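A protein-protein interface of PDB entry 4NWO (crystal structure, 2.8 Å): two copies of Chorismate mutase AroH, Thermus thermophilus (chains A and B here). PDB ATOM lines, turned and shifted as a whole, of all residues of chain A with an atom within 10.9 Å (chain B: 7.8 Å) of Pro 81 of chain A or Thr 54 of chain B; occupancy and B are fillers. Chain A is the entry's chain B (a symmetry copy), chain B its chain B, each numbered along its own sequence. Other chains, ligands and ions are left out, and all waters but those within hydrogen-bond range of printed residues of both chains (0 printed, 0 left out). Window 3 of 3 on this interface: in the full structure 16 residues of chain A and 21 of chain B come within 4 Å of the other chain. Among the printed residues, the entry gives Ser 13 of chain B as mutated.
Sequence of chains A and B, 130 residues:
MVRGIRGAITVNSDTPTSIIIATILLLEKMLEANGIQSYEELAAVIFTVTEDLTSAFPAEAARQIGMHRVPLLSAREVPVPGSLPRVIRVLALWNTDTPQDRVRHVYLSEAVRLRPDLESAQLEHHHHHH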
ATOM      1  N   THR A  50     -31.722  16.283 -24.330  1.00  0.00           N
ATOM      2  CA  THR A  50     -30.825  15.866 -25.398  1.00  0.00           C
ATOM      3  C   THR A  50     -30.329  17.083 -26.174  1.00  0.00           C
ATOM      4  O   THR A  50     -30.922  18.157 -26.111  1.00  0.00           O
ATOM      5  CB  THR A  50     -31.510  14.880 -26.360  1.00  0.00           C
ATOM      6  OG1 THR A  50     -32.775  15.409 -26.771  1.00  0.00           O
ATOM      7  CG2 THR A  50     -31.733  13.547 -25.673  1.00  0.00           C
ATOM      8  N   GLU A  51     -29.233  16.906 -26.906  1.00  0.00           N
ATOM      9  CA  GLU A  51     -28.553  18.008 -27.582  1.00  0.00           C
ATOM     10  C   GLU A  51     -29.364  18.627 -28.725  1.00  0.00           C
ATOM     11  O   GLU A  51     -29.048  19.722 -29.196  1.00  0.00           O
ATOM     12  CB  GLU A  51     -27.201  17.526 -28.114  1.00  0.00           C
ATOM     13  CG  GLU A  51     -26.229  18.636 -28.478  1.00  0.00           C
ATOM     14  N   ASP A  52     -30.408  17.937 -29.167  1.00  0.00           N
ATOM     15  CA  ASP A  52     -31.281  18.487 -30.200  1.00  0.00           C
ATOM     16  C   ASP A  52     -32.385  19.398 -29.645  1.00  0.00           C
ATOM     17  O   ASP A  52     -33.226  19.890 -30.396  1.00  0.00           O
ATOM     18  CB  ASP A  52     -31.875  17.351 -31.041  1.00  0.00           C
ATOM     19  CG  ASP A  52     -32.543  16.278 -30.200  1.00  0.00           C
ATOM     20  OD1 ASP A  52     -32.890  16.550 -29.033  1.00  0.00           O
ATOM     21  OD2 ASP A  52     -32.712  15.150 -30.711  1.00  0.00           O
ATOM     22  N   ARG A  76     -27.158  18.880 -19.761  1.00  0.00           N
ATOM     23  CA  ARG A  76     -27.272  18.248 -21.065  1.00  0.00           C
ATOM     24  C   ARG A  76     -27.040  16.747 -20.941  1.00  0.00           C
ATOM     25  O   ARG A  76     -26.146  16.302 -20.223  1.00  0.00           O
ATOM     26  CB  ARG A  76     -26.280  18.865 -22.054  1.00  0.00           C
ATOM     27  CG  ARG A  76     -26.372  20.379 -22.152  1.00  0.00           C
ATOM     28  N   GLU A  77     -27.855  15.978 -21.652  1.00  0.00           N
ATOM     29  CA  GLU A  77     -27.722  14.528 -21.693  1.00  0.00           C
ATOM     30  C   GLU A  77     -26.622  14.097 -22.649  1.00  0.00           C
ATOM     31  O   GLU A  77     -26.255  14.839 -23.562  1.00  0.00           O
ATOM     32  CB  GLU A  77     -29.046  13.878 -22.095  1.00  0.00           C
ATOM     33  N   VAL A  78     -26.094  12.899 -22.426  1.00  0.00           N
ATOM     34  CA  VAL A  78     -25.078  12.342 -23.307  1.00  0.00           C
ATOM     35  C   VAL A  78     -25.697  12.111 -24.679  1.00  0.00           C
ATOM     36  O   VAL A  78     -26.752  11.487 -24.789  1.00  0.00           O
ATOM     37  CB  VAL A  78     -24.531  11.022 -22.751  1.00  0.00           C
ATOM     38  CG1 VAL A  78     -23.378  10.514 -23.607  1.00  0.00           C
ATOM     39  CG2 VAL A  78     -24.081  11.217 -21.316  1.00  0.00           C
ATOM     40  N   PRO A  79     -25.038  12.613 -25.733  1.00  0.00           N
ATOM     41  CA  PRO A  79     -25.575  12.480 -27.090  1.00  0.00           C
ATOM     42  C   PRO A  79     -25.245  11.168 -27.801  1.00  0.00           C
ATOM     43  O   PRO A  79     -24.477  11.179 -28.765  1.00  0.00           O
ATOM     44  CB  PRO A  79     -24.910  13.651 -27.818  1.00  0.00           C
ATOM     45  CG  PRO A  79     -23.566  13.738 -27.155  1.00  0.00           C
ATOM     46  CD  PRO A  79     -23.855  13.489 -25.695  1.00  0.00           C
ATOM     47  N   VAL A  80     -25.816  10.057 -27.343  1.00  0.00           N
ATOM     48  CA  VAL A  80     -25.460   8.760 -27.905  1.00  0.00           C
ATOM     49  C   VAL A  80     -26.037   8.621 -29.315  1.00  0.00           C
ATOM     50  O   VAL A  80     -27.212   8.917 -29.533  1.00  0.00           O
ATOM     51  CB  VAL A  80     -25.975   7.601 -27.022  1.00  0.00           C
ATOM     52  CG1 VAL A  80     -25.750   6.259 -27.704  1.00  0.00           C
ATOM     53  CG2 VAL A  80     -25.309   7.637 -25.652  1.00  0.00           C
ATOM     54  N   PRO A  81     -25.206   8.201 -30.284  1.00  0.00           N
ATOM     55  CA  PRO A  81     -25.692   7.940 -31.645  1.00  0.00           C
ATOM     56  C   PRO A  81     -26.813   6.901 -31.676  1.00  0.00           C
ATOM     57  O   PRO A  81     -26.675   5.846 -31.056  1.00  0.00           O
ATOM     58  CB  PRO A  81     -24.452   7.420 -32.379  1.00  0.00           C
ATOM     59  CG  PRO A  81     -23.292   7.853 -31.571  1.00  0.00           C
ATOM     60  CD  PRO A  81     -23.746   8.056 -30.163  1.00  0.00           C
ATOM     61  N   GLY A  82     -27.895   7.189 -32.389  1.00  0.00           N
ATOM     62  CA  GLY A  82     -28.990   6.243 -32.517  1.00  0.00           C
ATOM     63  C   GLY A  82     -29.925   6.206 -31.324  1.00  0.00           C
ATOM     64  O   GLY A  82     -30.887   5.439 -31.307  1.00  0.00           O
ATOM     65  N   SER A  83     -29.644   7.030 -30.321  1.00  0.00           N
ATOM     66  CA  SER A  83     -30.478   7.069 -29.128  1.00  0.00           C
ATOM     67  C   SER A  83     -31.715   7.904 -29.415  1.00  0.00           C
ATOM     68  O   SER A  83     -31.745   8.657 -30.392  1.00  0.00           O
ATOM     69  CB  SER A  83     -29.707   7.638 -27.935  1.00  0.00           C
ATOM     70  OG  SER A  83     -29.285   8.966 -28.184  1.00  0.00           O
ATOM     71  N   LEU A  84     -32.737   7.762 -28.575  1.00  0.00           N
ATOM     72  CA  LEU A  84     -34.016   8.412 -28.823  1.00  0.00           C
ATOM     73  C   LEU A  84     -33.780   9.919 -28.846  1.00  0.00           C
ATOM     74  O   LEU A  84     -33.175  10.471 -27.925  1.00  0.00           O
ATOM     75  CB  LEU A  84     -35.038   8.021 -27.755  1.00  0.00           C
ATOM     76  CG  LEU A  84     -36.497   8.396 -28.002  1.00  0.00           C
ATOM     77  CD1 LEU A  84     -37.032   7.676 -29.231  1.00  0.00           C
ATOM     78  CD2 LEU A  84     -37.338   8.057 -26.782  1.00  0.00           C
ATOM     79  N   PRO A  85     -34.256  10.593 -29.900  1.00  0.00           N
ATOM     80  CA  PRO A  85     -34.144  12.050 -29.999  1.00  0.00           C
ATOM     81  C   PRO A  85     -35.136  12.830 -29.143  1.00  0.00           C
ATOM     82  O   PRO A  85     -36.202  12.317 -28.796  1.00  0.00           O
ATOM     83  CB  PRO A  85     -34.406  12.293 -31.485  1.00  0.00           C
ATOM     84  CG  PRO A  85     -35.436  11.272 -31.801  1.00  0.00           C
ATOM     85  CD  PRO A  85     -34.919  10.033 -31.091  1.00  0.00           C
ATOM     86  N   ARG A  89     -35.687  14.611 -19.619  1.00  0.00           N
ATOM     87  CA  ARG A  89     -35.657  13.717 -18.466  1.00  0.00           C
ATOM     88  C   ARG A  89     -35.692  14.481 -17.149  1.00  0.00           C
ATOM     89  O   ARG A  89     -35.119  15.563 -17.030  1.00  0.00           O
ATOM     90  CB  ARG A  89     -34.421  12.814 -18.507  1.00  0.00           C
ATOM     91  CG  ARG A  89     -34.399  11.830 -19.661  1.00  0.00           C
ATOM     92  CD  ARG A  89     -33.070  11.092 -19.731  1.00  0.00           C
ATOM     93  NE  ARG A  89     -33.126   9.955 -20.648  1.00  0.00           N
ATOM     94  CZ  ARG A  89     -32.879  10.029 -21.951  1.00  0.00           C
ATOM     95  NH1 ARG A  89     -32.574  11.195 -22.504  1.00  0.00           N
ATOM     96  NH2 ARG A  89     -32.908   8.932 -22.697  1.00  0.00           N
ATOM     97  N   SER B  13     -10.995   3.464 -24.795  1.00  0.00           N
ATOM     98  CA  SER B  13     -11.688   3.668 -26.064  1.00  0.00           C
ATOM     99  C   SER B  13     -13.168   3.988 -25.868  1.00  0.00           C
ATOM    100  O   SER B  13     -13.774   3.604 -24.867  1.00  0.00           O
ATOM    101  CB  SER B  13     -11.535   2.436 -26.964  1.00  0.00           C
ATOM    102  OG  SER B  13     -12.291   1.343 -26.468  1.00  0.00           O
ATOM    103  N   ASP B  14     -13.730   4.706 -26.834  1.00  0.00           N
ATOM    104  CA  ASP B  14     -15.146   5.047 -26.851  1.00  0.00           C
ATOM    105  C   ASP B  14     -15.952   3.948 -27.540  1.00  0.00           C
ATOM    106  O   ASP B  14     -16.389   4.107 -28.680  1.00  0.00           O
ATOM    107  CB  ASP B  14     -15.377   6.392 -27.542  1.00  0.00           C
ATOM    108  CG  ASP B  14     -16.826   6.844 -27.472  1.00  0.00           C
ATOM    109  OD1 ASP B  14     -17.604   6.250 -26.693  1.00  0.00           O
ATOM    110  OD2 ASP B  14     -17.186   7.799 -28.193  1.00  0.00           O
ATOM    111  N   THR B  15     -16.134   2.832 -26.843  1.00  0.00           N
ATOM    112  CA  THR B  15     -16.976   1.749 -27.335  1.00  0.00           C
ATOM    113  C   THR B  15     -17.966   1.401 -26.233  1.00  0.00           C
ATOM    114  O   THR B  15     -17.686   1.625 -25.057  1.00  0.00           O
ATOM    115  CB  THR B  15     -16.145   0.502 -27.718  1.00  0.00           C
ATOM    116  OG1 THR B  15     -15.514  -0.031 -26.547  1.00  0.00           O
ATOM    117  CG2 THR B  15     -15.077   0.862 -28.737  1.00  0.00           C
ATOM    118  N   PRO B  16     -19.134   0.853 -26.607  1.00  0.00           N
ATOM    119  CA  PRO B  16     -20.117   0.457 -25.590  1.00  0.00           C
ATOM    120  C   PRO B  16     -19.630  -0.605 -24.606  1.00  0.00           C
ATOM    121  O   PRO B  16     -19.902  -0.494 -23.410  1.00  0.00           O
ATOM    122  CB  PRO B  16     -21.271  -0.097 -26.433  1.00  0.00           C
ATOM    123  CG  PRO B  16     -21.146   0.618 -27.739  1.00  0.00           C
ATOM    124  CD  PRO B  16     -19.669   0.713 -27.971  1.00  0.00           C
ATOM    125  N   ILE B  19     -17.220   1.064 -21.951  1.00  0.00           N
ATOM    126  CA  ILE B  19     -17.889   1.978 -21.035  1.00  0.00           C
ATOM    127  C   ILE B  19     -18.768   1.223 -20.042  1.00  0.00           C
ATOM    128  O   ILE B  19     -18.750   1.513 -18.846  1.00  0.00           O
ATOM    129  CB  ILE B  19     -18.761   3.001 -21.803  1.00  0.00           C
ATOM    130  CG1 ILE B  19     -17.883   3.974 -22.590  1.00  0.00           C
ATOM    131  CG2 ILE B  19     -19.678   3.757 -20.850  1.00  0.00           C
ATOM    132  CD1 ILE B  19     -18.654   4.815 -23.588  1.00  0.00           C
ATOM    133  N   VAL B  49     -20.104  11.769 -18.132  1.00  0.00           N
ATOM    134  CA  VAL B  49     -19.042  11.311 -19.020  1.00  0.00           C
ATOM    135  C   VAL B  49     -18.392  12.506 -19.701  1.00  0.00           C
ATOM    136  O   VAL B  49     -19.055  13.505 -19.984  1.00  0.00           O
ATOM    137  CB  VAL B  49     -19.542  10.316 -20.084  1.00  0.00           C
ATOM    138  CG1 VAL B  49     -19.998   9.025 -19.430  1.00  0.00           C
ATOM    139  CG2 VAL B  49     -20.645  10.928 -20.919  1.00  0.00           C
ATOM    140  N   THR B  50     -17.091  12.413 -19.947  1.00  0.00           N
ATOM    141  CA  THR B  50     -16.404  13.430 -20.729  1.00  0.00           C
ATOM    142  C   THR B  50     -16.879  13.390 -22.180  1.00  0.00           C
ATOM    143  O   THR B  50     -17.449  12.398 -22.629  1.00  0.00           O
ATOM    144  CB  THR B  50     -14.877  13.248 -20.678  1.00  0.00           C
ATOM    145  OG1 THR B  50     -14.544  11.890 -20.980  1.00  0.00           O
ATOM    146  CG2 THR B  50     -14.355  13.588 -19.296  1.00  0.00           C
ATOM    147  N   GLU B  51     -16.642  14.477 -22.906  1.00  0.00           N
ATOM    148  CA  GLU B  51     -17.166  14.648 -24.259  1.00  0.00           C
ATOM    149  C   GLU B  51     -16.563  13.683 -25.283  1.00  0.00           C
ATOM    150  O   GLU B  51     -17.096  13.522 -26.383  1.00  0.00           O
ATOM    151  CB  GLU B  51     -16.939  16.092 -24.716  1.00  0.00           C
ATOM    152  CG  GLU B  51     -17.772  16.517 -25.915  1.00  0.00           C
ATOM    153  N   ASP B  52     -15.458  13.038 -24.927  1.00  0.00           N
ATOM    154  CA  ASP B  52     -14.861  12.042 -25.812  1.00  0.00           C
ATOM    155  C   ASP B  52     -15.475  10.643 -25.660  1.00  0.00           C
ATOM    156  O   ASP B  52     -15.033   9.693 -26.306  1.00  0.00           O
ATOM    157  CB  ASP B  52     -13.342  12.003 -25.602  1.00  0.00           C
ATOM    158  CG  ASP B  52     -12.949  11.825 -24.146  1.00  0.00           C
ATOM    159  OD1 ASP B  52     -13.786  11.365 -23.344  1.00  0.00           O
ATOM    160  OD2 ASP B  52     -11.795  12.159 -23.803  1.00  0.00           O
ATOM    161  N   LEU B  53     -16.501  10.524 -24.822  1.00  0.00           N
ATOM    162  CA  LEU B  53     -17.231   9.264 -24.676  1.00  0.00           C
ATOM    163  C   LEU B  53     -18.693   9.498 -25.041  1.00  0.00           C
ATOM    164  O   LEU B  53     -19.444  10.087 -24.267  1.00  0.00           O
ATOM    165  CB  LEU B  53     -17.119   8.731 -23.249  1.00  0.00           C
ATOM    166  CG  LEU B  53     -15.718   8.379 -22.747  1.00  0.00           C
ATOM    167  CD1 LEU B  53     -15.754   7.969 -21.277  1.00  0.00           C
ATOM    168  CD2 LEU B  53     -15.102   7.287 -23.606  1.00  0.00           C
ATOM    169  N   THR B  54     -19.097   9.030 -26.220  1.00  0.00           N
ATOM    170  CA  THR B  54     -20.493   9.140 -26.639  1.00  0.00           C
ATOM    171  C   THR B  54     -21.220   7.855 -27.052  1.00  0.00           C
ATOM    172  O   THR B  54     -22.405   7.903 -27.369  1.00  0.00           O
ATOM    173  CB  THR B  54     -20.607  10.119 -27.827  1.00  0.00           C
ATOM    174  OG1 THR B  54     -19.752   9.681 -28.889  1.00  0.00           O
ATOM    175  CG2 THR B  54     -20.206  11.527 -27.409  1.00  0.00           C
ATOM    176  N   SER B  55     -20.548   6.709 -27.032  1.00  0.00           N
ATOM    177  CA  SER B  55     -21.122   5.515 -27.659  1.00  0.00           C
ATOM    178  C   SER B  55     -22.170   4.777 -26.825  1.00  0.00           C
ATOM    179  O   SER B  55     -22.898   3.936 -27.350  1.00  0.00           O
ATOM    180  CB  SER B  55     -20.008   4.534 -28.023  1.00  0.00           C
ATOM    181  OG  SER B  55     -19.432   3.973 -26.854  1.00  0.00           O
ATOM    182  N   ALA B  56     -22.256   5.086 -25.535  1.00  0.00           N
ATOM    183  CA  ALA B  56     -23.112   4.309 -24.643  1.00  0.00           C
ATOM    184  C   ALA B  56     -23.578   5.091 -23.419  1.00  0.00           C
ATOM    185  O   ALA B  56     -22.931   6.046 -22.992  1.00  0.00           O
ATOM    186  CB  ALA B  56     -22.390   3.044 -24.204  1.00  0.00           C
ATOM    187  N   PHE B  57     -24.711   4.675 -22.861  1.00  0.00           N
ATOM    188  CA  PHE B  57     -25.172   5.189 -21.575  1.00  0.00           C
ATOM    189  C   PHE B  57     -24.599   4.341 -20.441  1.00  0.00           C
ATOM    190  O   PHE B  57     -24.783   3.126 -20.418  1.00  0.00           O
ATOM    191  CB  PHE B  57     -26.703   5.210 -21.484  1.00  0.00           C
ATOM    192  CG  PHE B  57     -27.366   6.219 -22.385  1.00  0.00           C
ATOM    193  CD1 PHE B  57     -27.274   7.577 -22.119  1.00  0.00           C
ATOM    194  CD2 PHE B  57     -28.121   5.806 -23.472  1.00  0.00           C
ATOM    195  CE1 PHE B  57     -27.895   8.505 -22.938  1.00  0.00           C
ATOM    196  CE2 PHE B  57     -28.746   6.728 -24.292  1.00  0.00           C
ATOM    197  CZ  PHE B  57     -28.634   8.078 -24.025  1.00  0.00           C
ATOM    198  N   ARG B  76     -23.369  15.342 -19.266  1.00  0.00           N
ATOM    199  CA  ARG B  76     -22.046  15.538 -19.834  1.00  0.00           C
ATOM    200  C   ARG B  76     -21.191  16.376 -18.891  1.00  0.00           C
ATOM    201  O   ARG B  76     -21.659  17.355 -18.313  1.00  0.00           O
ATOM    202  CB  ARG B  76     -22.139  16.205 -21.209  1.00  0.00           C
ATOM    203  CG  ARG B  76     -23.068  15.488 -22.177  1.00  0.00           C
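The backbone carbonyl oxygen (O) of Arg 76 of chain A sits at hydrogen-bond distance from the backbone NH (N) of Arg 76 of chain B, at 3.1 Å.
The side-chain carboxylate of Asp 14 of chain B is in hydrogen-bond range of the backbone NH of Thr 54 of chain B, 3.0 Å away. OG of Ser 55 of chain B sits close to O of Thr 15 of chain B (3.4 Å). OD1 of Asp 14 of chain B is in hydrogen-bond range of OG of Ser 55 of chain B (2.9 Å). The backbone carbonyl oxygen (O) of Val 80 of chain A sits at hydrogen-bond distance from the side-chain hydroxyl (OG) of Ser 83 of chain A (2.5 Å).
Among the printed residues, merely in contact across the chains: Pro 81 of chain A with Thr 54 of chain B (3.1 Å), Val 80 of chain A with Thr 54 of chain B (3.2 Å), Val 78 of chain A with Val 49 of chain B (3.5 Å), Glu 77 of chain A with Arg 76 of chain B (3.5 Å), Val 78 of chain A with Phe 57 of chain B (3.7 Å), Val 80 of chain A with Ser 55 of chain B (3.7 Å), Val 80 of chain A with Phe 57 of chain B (3.7 Å), Val 80 of chain A with Ala 56 of chain B (3.8 Å), Ser 83 of chain A with Phe 57 of chain B (3.9 Å) and Val 78 of chain A with Arg 76 of chain B (3.9 Å).
Of the printed residues of chain B, Arg 76 of chain A touches Arg 76. Of chain B, only Thr 54, Ser 55, Ala 56 and Phe 57 come within 4 Å of Val 80 of chain A. Of chain B, only Thr 54 (3.1 Å) comes within 4 Å of Pro 81 of chain A. Printed residues of chain B within 4 Å of Ser 83 of chain A: Phe 57 (3.9 Å). Of the printed residues of chain A, Val 49 of chain B touches Val 78. No residue of chain A comes within 4 Å of Glu 51 of chain B. Thr 54 of chain B touches just these residues of chain A: Val 80 (3.2 Å) and Pro 81 (3.1 Å). Of the printed residues of chain A, Arg 76 of chain B touches Arg 76 (3.1 Å), Glu 77 (3.5 Å) and Val 78 (3.9 Å). The nearest printed residue of chain A that does not touch Val 49 of chain B is Pro 79 of chain A (6.3 Å).
Of the 15 printed residues of chain B, 6 touch a printed residue of chain A. Hydrophobic or aromatic side chains of chain B within 4 Å of the printed part of chain A: Val 49 and Phe 57. Of the 14 printed residues of chain A, 6 touch a printed residue of chain B. Hydrophobic or aromatic side chains of chain A within 4 Å of the printed part of chain B: Val 78, Val 80 and Pro 81. Among the printed residues, 11 pairs touch across the chains. Among the printed residues, no Asp or Glu carboxylate lies within 4 Å of a Lys or Arg side-chain nitrogen of the other chain.
Arg 76 of chain B touches its own counterpart, Arg 76 of chain A. Positions printed for both chains: 50, 51, 52 and 76.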
